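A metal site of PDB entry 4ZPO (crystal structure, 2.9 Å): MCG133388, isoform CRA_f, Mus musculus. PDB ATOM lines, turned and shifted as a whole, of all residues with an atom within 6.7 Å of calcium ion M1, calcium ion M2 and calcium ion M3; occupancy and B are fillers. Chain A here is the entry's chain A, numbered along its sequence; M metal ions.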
ATOM      1  N   GLU A 115       6.564  -8.753  10.164  1.00  0.00           N
ATOM      2  CA  GLU A 115       6.165  -8.142  11.423  1.00  0.00           C
ATOM      3  C   GLU A 115       4.911  -7.281  11.234  1.00  0.00           C
ATOM      4  O   GLU A 115       4.217  -6.961  12.200  1.00  0.00           O
ATOM      5  CB  GLU A 115       7.304  -7.299  11.988  1.00  0.00           C
ATOM      6  CG  GLU A 115       7.123  -6.839  13.417  1.00  0.00           C
ATOM      7  CD  GLU A 115       8.299  -6.024  13.903  1.00  0.00           C
ATOM      8  OE1 GLU A 115       9.232  -5.789  13.113  1.00  0.00           O
ATOM      9  OE2 GLU A 115       8.283  -5.615  15.086  1.00  0.00           O
ATOM     10  N   GLN A 170      -0.922  -8.764  16.860  1.00  0.00           N
ATOM     11  CA  GLN A 170       0.182  -8.339  16.002  1.00  0.00           C
ATOM     12  C   GLN A 170       1.530  -8.812  16.537  1.00  0.00           C
ATOM     13  O   GLN A 170       1.826  -8.654  17.724  1.00  0.00           O
ATOM     14  CB  GLN A 170       0.184  -6.825  15.851  1.00  0.00           C
ATOM     15  CG  GLN A 170       1.334  -6.279  15.017  1.00  0.00           C
ATOM     16  CD  GLN A 170       1.355  -6.843  13.607  1.00  0.00           C
ATOM     17  OE1 GLN A 170       1.889  -7.930  13.370  1.00  0.00           O
ATOM     18  NE2 GLN A 170       0.775  -6.111  12.666  1.00  0.00           N
ATOM     19  N   LEU A 171       2.342  -9.374  15.655  1.00  0.00           N
ATOM     20  CA  LEU A 171       3.672  -9.843  16.030  1.00  0.00           C
ATOM     21  C   LEU A 171       4.625  -8.663  16.217  1.00  0.00           C
ATOM     22  O   LEU A 171       4.445  -7.607  15.615  1.00  0.00           O
ATOM     23  CB  LEU A 171       4.225 -10.789  14.959  1.00  0.00           C
ATOM     24  CG  LEU A 171       3.369 -12.008  14.615  1.00  0.00           C
ATOM     25  CD1 LEU A 171       3.995 -12.796  13.480  1.00  0.00           C
ATOM     26  CD2 LEU A 171       3.166 -12.885  15.839  1.00  0.00           C
ATOM     27  N   ASP A 172       5.634  -8.852  17.061  1.00  0.00           N
ATOM     28  CA  ASP A 172       6.620  -7.812  17.315  1.00  0.00           C
ATOM     29  C   ASP A 172       8.009  -8.416  17.461  1.00  0.00           C
ATOM     30  O   ASP A 172       8.330  -9.042  18.472  1.00  0.00           O
ATOM     31  CB  ASP A 172       6.254  -7.022  18.568  1.00  0.00           C
ATOM     32  CG  ASP A 172       7.192  -5.859  18.825  1.00  0.00           C
ATOM     33  OD1 ASP A 172       7.814  -5.372  17.869  1.00  0.00           O
ATOM     34  OD2 ASP A 172       7.303  -5.424  20.000  1.00  0.00           O
ATOM     35  N   ARG A 173       8.847  -8.212  16.440  1.00  0.00           N
ATOM     36  CA  ARG A 173      10.193  -8.774  16.413  1.00  0.00           C
ATOM     37  C   ARG A 173      11.054  -8.251  17.554  1.00  0.00           C
ATOM     38  O   ARG A 173      11.967  -8.925  18.026  1.00  0.00           O
ATOM     39  CB  ARG A 173      10.869  -8.462  15.069  1.00  0.00           C
ATOM     40  CG  ARG A 173      12.241  -9.074  14.920  1.00  0.00           C
ATOM     41  CD  ARG A 173      13.065  -8.339  13.882  1.00  0.00           C
ATOM     42  NE  ARG A 173      14.483  -8.330  14.242  1.00  0.00           N
ATOM     43  CZ  ARG A 173      15.047  -7.406  15.004  1.00  0.00           C
ATOM     44  NH1 ARG A 173      14.321  -6.406  15.489  1.00  0.00           N
ATOM     45  NH2 ARG A 173      16.340  -7.474  15.292  1.00  0.00           N
ATOM     46  N   GLU A 174      10.756  -7.038  18.023  1.00  0.00           N
ATOM     47  CA  GLU A 174      11.526  -6.416  19.096  1.00  0.00           C
ATOM     48  C   GLU A 174      11.338  -7.126  20.435  1.00  0.00           C
ATOM     49  O   GLU A 174      12.152  -6.974  21.340  1.00  0.00           O
ATOM     50  CB  GLU A 174      11.165  -4.938  19.225  1.00  0.00           C
ATOM     51  CG  GLU A 174      11.861  -4.027  18.216  1.00  0.00           C
ATOM     52  CD  GLU A 174      11.342  -4.192  16.805  1.00  0.00           C
ATOM     53  OE1 GLU A 174      12.158  -4.389  15.887  1.00  0.00           O
ATOM     54  OE2 GLU A 174      10.113  -4.119  16.613  1.00  0.00           O
ATOM     55  N   LEU A 204       9.917 -11.671  10.422  1.00  0.00           N
ATOM     56  CA  LEU A 204      10.770 -10.808   9.604  1.00  0.00           C
ATOM     57  C   LEU A 204      10.648  -9.362  10.063  1.00  0.00           C
ATOM     58  O   LEU A 204       9.585  -8.938  10.520  1.00  0.00           O
ATOM     59  CB  LEU A 204      10.385 -10.929   8.127  1.00  0.00           C
ATOM     60  CG  LEU A 204      10.530 -12.317   7.512  1.00  0.00           C
ATOM     61  CD1 LEU A 204      10.075 -12.335   6.058  1.00  0.00           C
ATOM     62  CD2 LEU A 204      11.967 -12.814   7.630  1.00  0.00           C
ATOM     63  N   ASP A 205      11.730  -8.611   9.948  1.00  0.00           N
ATOM     64  CA  ASP A 205      11.773  -7.249  10.470  1.00  0.00           C
ATOM     65  C   ASP A 205      11.028  -6.246   9.596  1.00  0.00           C
ATOM     66  O   ASP A 205      11.059  -6.321   8.363  1.00  0.00           O
ATOM     67  CB  ASP A 205      13.214  -6.786  10.644  1.00  0.00           C
ATOM     68  CG  ASP A 205      13.318  -5.454  11.369  1.00  0.00           C
ATOM     69  OD1 ASP A 205      12.562  -5.245  12.334  1.00  0.00           O
ATOM     70  OD2 ASP A 205      14.155  -4.612  10.956  1.00  0.00           O
ATOM     71  N   VAL A 206      10.351  -5.310  10.250  1.00  0.00           N
ATOM     72  CA  VAL A 206       9.703  -4.189   9.579  1.00  0.00           C
ATOM     73  C   VAL A 206      10.057  -2.914  10.343  1.00  0.00           C
ATOM     74  O   VAL A 206      10.080  -2.921  11.570  1.00  0.00           O
ATOM     75  CB  VAL A 206       8.167  -4.360   9.520  1.00  0.00           C
ATOM     76  CG1 VAL A 206       7.493  -3.075   9.049  1.00  0.00           C
ATOM     77  CG2 VAL A 206       7.789  -5.519   8.623  1.00  0.00           C
ATOM     78  N   ASN A 207      10.368  -1.839   9.618  1.00  0.00           N
ATOM     79  CA  ASN A 207      10.706  -0.576  10.270  1.00  0.00           C
ATOM     80  C   ASN A 207       9.499  -0.007  11.017  1.00  0.00           C
ATOM     81  O   ASN A 207       8.788   0.849  10.493  1.00  0.00           O
ATOM     82  CB  ASN A 207      11.225   0.435   9.252  1.00  0.00           C
ATOM     83  CG  ASN A 207      12.009   1.565   9.904  1.00  0.00           C
ATOM     84  OD1 ASN A 207      11.747   1.948  11.044  1.00  0.00           O
ATOM     85  ND2 ASN A 207      12.977   2.102   9.188  1.00  0.00           N
ATOM     86  N   ASP A 208       9.278  -0.488  12.233  1.00  0.00           N
ATOM     87  CA  ASP A 208       8.163  -0.019  13.047  1.00  0.00           C
ATOM     88  C   ASP A 208       8.664   0.685  14.310  1.00  0.00           C
ATOM     89  O   ASP A 208       7.966   0.742  15.317  1.00  0.00           O
ATOM     90  CB  ASP A 208       7.249  -1.191  13.427  1.00  0.00           C
ATOM     91  CG  ASP A 208       7.915  -2.177  14.372  1.00  0.00           C
ATOM     92  OD1 ASP A 208       8.666  -3.049  13.894  1.00  0.00           O
ATOM     93  OD2 ASP A 208       7.681  -2.080  15.597  1.00  0.00           O
ATOM     94  N   ASN A 209       9.881   1.206  14.239  1.00  0.00           N
ATOM     95  CA  ASN A 209      10.454   1.957  15.349  1.00  0.00           C
ATOM     96  C   ASN A 209      11.223   3.181  14.879  1.00  0.00           C
ATOM     97  O   ASN A 209      11.901   3.141  13.846  1.00  0.00           O
ATOM     98  CB  ASN A 209      11.359   1.060  16.184  1.00  0.00           C
ATOM     99  CG  ASN A 209      10.588   0.197  17.178  1.00  0.00           C
ATOM    100  OD1 ASN A 209      10.116  -0.884  16.830  1.00  0.00           O
ATOM    101  ND2 ASN A 209      10.469   0.683  18.402  1.00  0.00           N
ATOM    102  N   ALA A 210      11.099   4.268  15.628  1.00  0.00           N
ATOM    103  CA  ALA A 210      11.826   5.489  15.324  1.00  0.00           C
ATOM    104  C   ALA A 210      12.981   5.666  16.293  1.00  0.00           C
ATOM    105  O   ALA A 210      12.875   5.281  17.462  1.00  0.00           O
ATOM    106  CB  ALA A 210      10.901   6.694  15.362  1.00  0.00           C
ATOM    107  N   PRO A 211      14.099   6.241  15.823  1.00  0.00           N
ATOM    108  CA  PRO A 211      15.242   6.526  16.697  1.00  0.00           C
ATOM    109  C   PRO A 211      14.833   7.407  17.877  1.00  0.00           C
ATOM    110  O   PRO A 211      13.973   8.264  17.722  1.00  0.00           O
ATOM    111  CB  PRO A 211      16.222   7.254  15.776  1.00  0.00           C
ATOM    112  CG  PRO A 211      15.873   6.769  14.412  1.00  0.00           C
ATOM    113  CD  PRO A 211      14.385   6.590  14.418  1.00  0.00           C
ATOM    114  N   ASP A 239      18.027   2.591  18.170  1.00  0.00           N
ATOM    115  CA  ASP A 239      16.984   2.068  17.311  1.00  0.00           C
ATOM    116  C   ASP A 239      16.990   0.545  17.369  1.00  0.00           C
ATOM    117  O   ASP A 239      17.968  -0.096  16.967  1.00  0.00           O
ATOM    118  CB  ASP A 239      17.169   2.555  15.876  1.00  0.00           C
ATOM    119  CG  ASP A 239      15.920   2.390  15.039  1.00  0.00           C
ATOM    120  OD1 ASP A 239      15.624   1.250  14.626  1.00  0.00           O
ATOM    121  OD2 ASP A 239      15.222   3.400  14.802  1.00  0.00           O
ATOM    122  N   PRO A 240      15.902  -0.053  17.873  1.00  0.00           N
ATOM    123  CA  PRO A 240      15.803  -1.498  18.126  1.00  0.00           C
ATOM    124  C   PRO A 240      15.604  -2.335  16.856  1.00  0.00           C
ATOM    125  O   PRO A 240      15.658  -3.562  16.935  1.00  0.00           O
ATOM    126  CB  PRO A 240      14.592  -1.601  19.043  1.00  0.00           C
ATOM    127  CG  PRO A 240      13.724  -0.461  18.639  1.00  0.00           C
ATOM    128  CD  PRO A 240      14.671   0.662  18.269  1.00  0.00           C
ATOM    129  N   ASP A 241      15.355  -1.687  15.729  1.00  0.00           N
ATOM    130  CA  ASP A 241      15.089  -2.411  14.483  1.00  0.00           C
ATOM    131  C   ASP A 241      16.355  -3.059  13.932  1.00  0.00           C
ATOM    132  O   ASP A 241      17.471  -2.712  14.311  1.00  0.00           O
ATOM    133  CB  ASP A 241      14.475  -1.473  13.445  1.00  0.00           C
ATOM    134  CG  ASP A 241      13.074  -1.040  13.813  1.00  0.00           C
ATOM    135  OD1 ASP A 241      12.406  -1.760  14.585  1.00  0.00           O
ATOM    136  OD2 ASP A 241      12.620   0.017  13.317  1.00  0.00           O
ATOM    137  N   GLU A 242      16.157  -4.018  13.029  1.00  0.00           N
ATOM    138  CA  GLU A 242      17.251  -4.830  12.499  1.00  0.00           C
ATOM    139  C   GLU A 242      17.865  -4.248  11.233  1.00  0.00           C
ATOM    140  O   GLU A 242      17.156  -3.708  10.375  1.00  0.00           O
ATOM    141  CB  GLU A 242      16.753  -6.256  12.222  1.00  0.00           C
ATOM    142  CG  GLU A 242      17.813  -7.219  11.722  1.00  0.00           C
ATOM    143  CD  GLU A 242      17.252  -8.588  11.429  1.00  0.00           C
ATOM    144  OE1 GLU A 242      16.021  -8.773  11.543  1.00  0.00           O
ATOM    145  OE2 GLU A 242      18.042  -9.495  11.074  1.00  0.00           O
ATOM    146  N   THR A 244      19.612  -2.090   8.400  1.00  0.00           N
ATOM    147  CA  THR A 244      19.563  -0.687   8.002  1.00  0.00           C
ATOM    148  C   THR A 244      18.411   0.044   8.688  1.00  0.00           C
ATOM    149  O   THR A 244      18.456   1.257   8.862  1.00  0.00           O
ATOM    150  CB  THR A 244      19.416  -0.541   6.473  1.00  0.00           C
ATOM    151  OG1 THR A 244      18.201  -1.171   6.050  1.00  0.00           O
ATOM    152  CG2 THR A 244      20.594  -1.181   5.769  1.00  0.00           C
ATOM    153  N   ASN A 245      17.394  -0.707   9.081  1.00  0.00           N
ATOM    154  CA  ASN A 245      16.266  -0.142   9.810  1.00  0.00           C
ATOM    155  C   ASN A 245      16.673   0.306  11.204  1.00  0.00           C
ATOM    156  O   ASN A 245      15.965   1.085  11.846  1.00  0.00           O
ATOM    157  CB  ASN A 245      15.121  -1.153   9.890  1.00  0.00           C
ATOM    158  CG  ASN A 245      14.476  -1.436   8.554  1.00  0.00           C
ATOM    159  OD1 ASN A 245      15.015  -1.064   7.505  1.00  0.00           O
ATOM    160  ND2 ASN A 245      13.328  -2.098   8.566  1.00  0.00           N
ATOM    161  N   GLY A 246      17.816  -0.179  11.675  1.00  0.00           N
ATOM    162  CA  GLY A 246      18.315   0.157  12.992  1.00  0.00           C
ATOM    163  C   GLY A 246      19.439   1.173  12.986  1.00  0.00           C
ATOM    164  O   GLY A 246      19.704   1.827  13.987  1.00  0.00           O
ATOM    165  N   GLN A 247      20.116   1.303  11.847  1.00  0.00           N
ATOM    166  CA  GLN A 247      21.195   2.274  11.706  1.00  0.00           C
ATOM    167  C   GLN A 247      20.629   3.671  11.455  1.00  0.00           C
ATOM    168  O   GLN A 247      19.594   3.818  10.800  1.00  0.00           O
ATOM    169  CB  GLN A 247      22.151   1.871  10.580  1.00  0.00           C
ATOM    170  CG  GLN A 247      23.020   0.667  10.924  1.00  0.00           C
ATOM    171  CD  GLN A 247      24.043   0.366   9.850  1.00  0.00           C
ATOM    172  OE1 GLN A 247      23.710   0.224   8.669  1.00  0.00           O
ATOM    173  NE2 GLN A 247      25.305   0.279  10.249  1.00  0.00           N
ATOM    174  N   ASP A 295      16.541   7.704  10.320  1.00  0.00           N
ATOM    175  CA  ASP A 295      16.671   6.267  10.085  1.00  0.00           C
ATOM    176  C   ASP A 295      17.168   5.997   8.677  1.00  0.00           C
ATOM    177  O   ASP A 295      17.295   6.916   7.863  1.00  0.00           O
ATOM    178  CB  ASP A 295      15.336   5.562  10.321  1.00  0.00           C
ATOM    179  CG  ASP A 295      15.505   4.144  10.797  1.00  0.00           C
ATOM    180  OD1 ASP A 295      16.635   3.638  10.768  1.00  0.00           O
ATOM    181  OD2 ASP A 295      14.482   3.530  11.182  1.00  0.00           O
ATOM    182  N   GLN A 296      17.456   4.732   8.374  1.00  0.00           N
ATOM    183  CA  GLN A 296      17.898   4.350   7.034  1.00  0.00           C
ATOM    184  C   GLN A 296      16.953   3.332   6.404  1.00  0.00           C
ATOM    185  O   GLN A 296      17.277   2.715   5.385  1.00  0.00           O
ATOM    186  CB  GLN A 296      19.314   3.785   7.082  1.00  0.00           C
ATOM    187  CG  GLN A 296      20.385   4.811   7.387  1.00  0.00           C
ATOM    188  CD  GLN A 296      21.787   4.258   7.214  1.00  0.00           C
ATOM    189  OE1 GLN A 296      21.971   3.126   6.778  1.00  0.00           O
ATOM    190  NE2 GLN A 296      22.790   5.066   7.552  1.00  0.00           N
ATOM    191  N   GLY A 297      15.784   3.162   7.003  1.00  0.00           N
ATOM    192  CA  GLY A 297      14.797   2.231   6.481  1.00  0.00           C
ATOM    193  C   GLY A 297      13.816   2.901   5.536  1.00  0.00           C
ATOM    194  O   GLY A 297      13.855   4.105   5.333  1.00  0.00           O
ATOM    195  N   MET A 301      12.332   6.698   9.542  1.00  0.00           N
ATOM    196  CA  MET A 301      11.834   7.214  10.815  1.00  0.00           C
ATOM    197  C   MET A 301      12.840   8.205  11.395  1.00  0.00           C
ATOM    198  O   MET A 301      13.986   8.268  10.945  1.00  0.00           O
ATOM    199  CB  MET A 301      11.593   6.069  11.798  1.00  0.00           C
ATOM    200  CG  MET A 301      10.633   4.994  11.302  1.00  0.00           C
ATOM    201  SD  MET A 301       8.963   5.614  11.012  1.00  0.00           S
ATOM    202  CE  MET A 301       8.037   4.086  11.002  1.00  0.00           C
HETATM  203 CA    CA M   1       6.549  -4.173  16.117  1.00  0.00          CA
HETATM  204 CA    CA M   2      11.009  -3.864  13.696  1.00  0.00          CA
HETATM  205 CA    CA M   3      13.924   2.079  12.999  1.00  0.00          CA
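The side-chain carboxylate (OD1) of Asp 172 sits close to the backbone NH (N) of Glu 174, 3.4 Å away. The side-chain carboxylate (OD2) of Asp 208 lies close to the side-chain amide oxygen (OD1) of Asn 209 (3.0 Å). O of Met 301 is in hydrogen-bond range of N of Asp 295, at 2.7 Å. The side-chain carboxylate of Asp 295 sits close to the side-chain amide nitrogen of Asn 207 (2.9 Å). OE2 of Glu 115 lies close to N of Arg 173 (3.0 Å). OE1 of Glu 174 sits close to NH1 of Arg 173. OD1 of Asp 205 sits close to NH1 of Arg 173. The side-chain amide oxygen (OD1) of Asn 207 lies close to the side-chain carboxylate (OD2) of Asp 241.
Four residues have an atom within 4 Å of calcium ion M1: Glu 115, Asp 172, Glu 174 and Asp 208.
Of the 26 residues printed, 6 come within 4 Å of calcium ion M2.
Within 4 Å of calcium ion M3: Asn 207, Asn 209, Asp 239, Asp 241, Asn 245 and Asp 295.
Calcium ion M1 is bound by OD2 of Asp 208 (2.4 Å), OD1 of Asp 172 (2.5 Å) and OE2 of Glu 115 (2.5 Å). Calcium ion M1 has three donor atoms within binding distance.
Calcium ion M2 is bound by OD1 of Asp 205 (2.5 Å), OD1 of Asp 208 (2.5 Å), O of Val 206 (2.5 Å), OE1 of Glu 174 (2.5 Å), OD1 of Asp 241 (2.7 Å) and OE1 of Glu 115 (2.7 Å). Calcium ion M2 has six donor atoms within binding distance. Slightly farther from calcium ion M2 lies OE2 of Glu 174 (3.1 Å).
OD2 of Asp 295 binds calcium ion M3 (2.4 Å). The backbone carbonyl oxygen (O) of Asn 209 is bound to calcium ion M3, at 2.4 Å. The side-chain carboxylate (OD2) of Asp 241 binds calcium ion M3 (2.5 Å). OD1 of Asp 239 is bound to calcium ion M3, 2.5 Å away. The backbone carbonyl oxygen (O) of Asn 245 is bound to calcium ion M3, at 2.5 Å. Calcium ion M3 is bound by OD2 of Asp 239 (2.6 Å). Slightly farther from calcium ion M3 lies the side-chain amide oxygen (OD1) of Asn 207 (2.9 Å).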
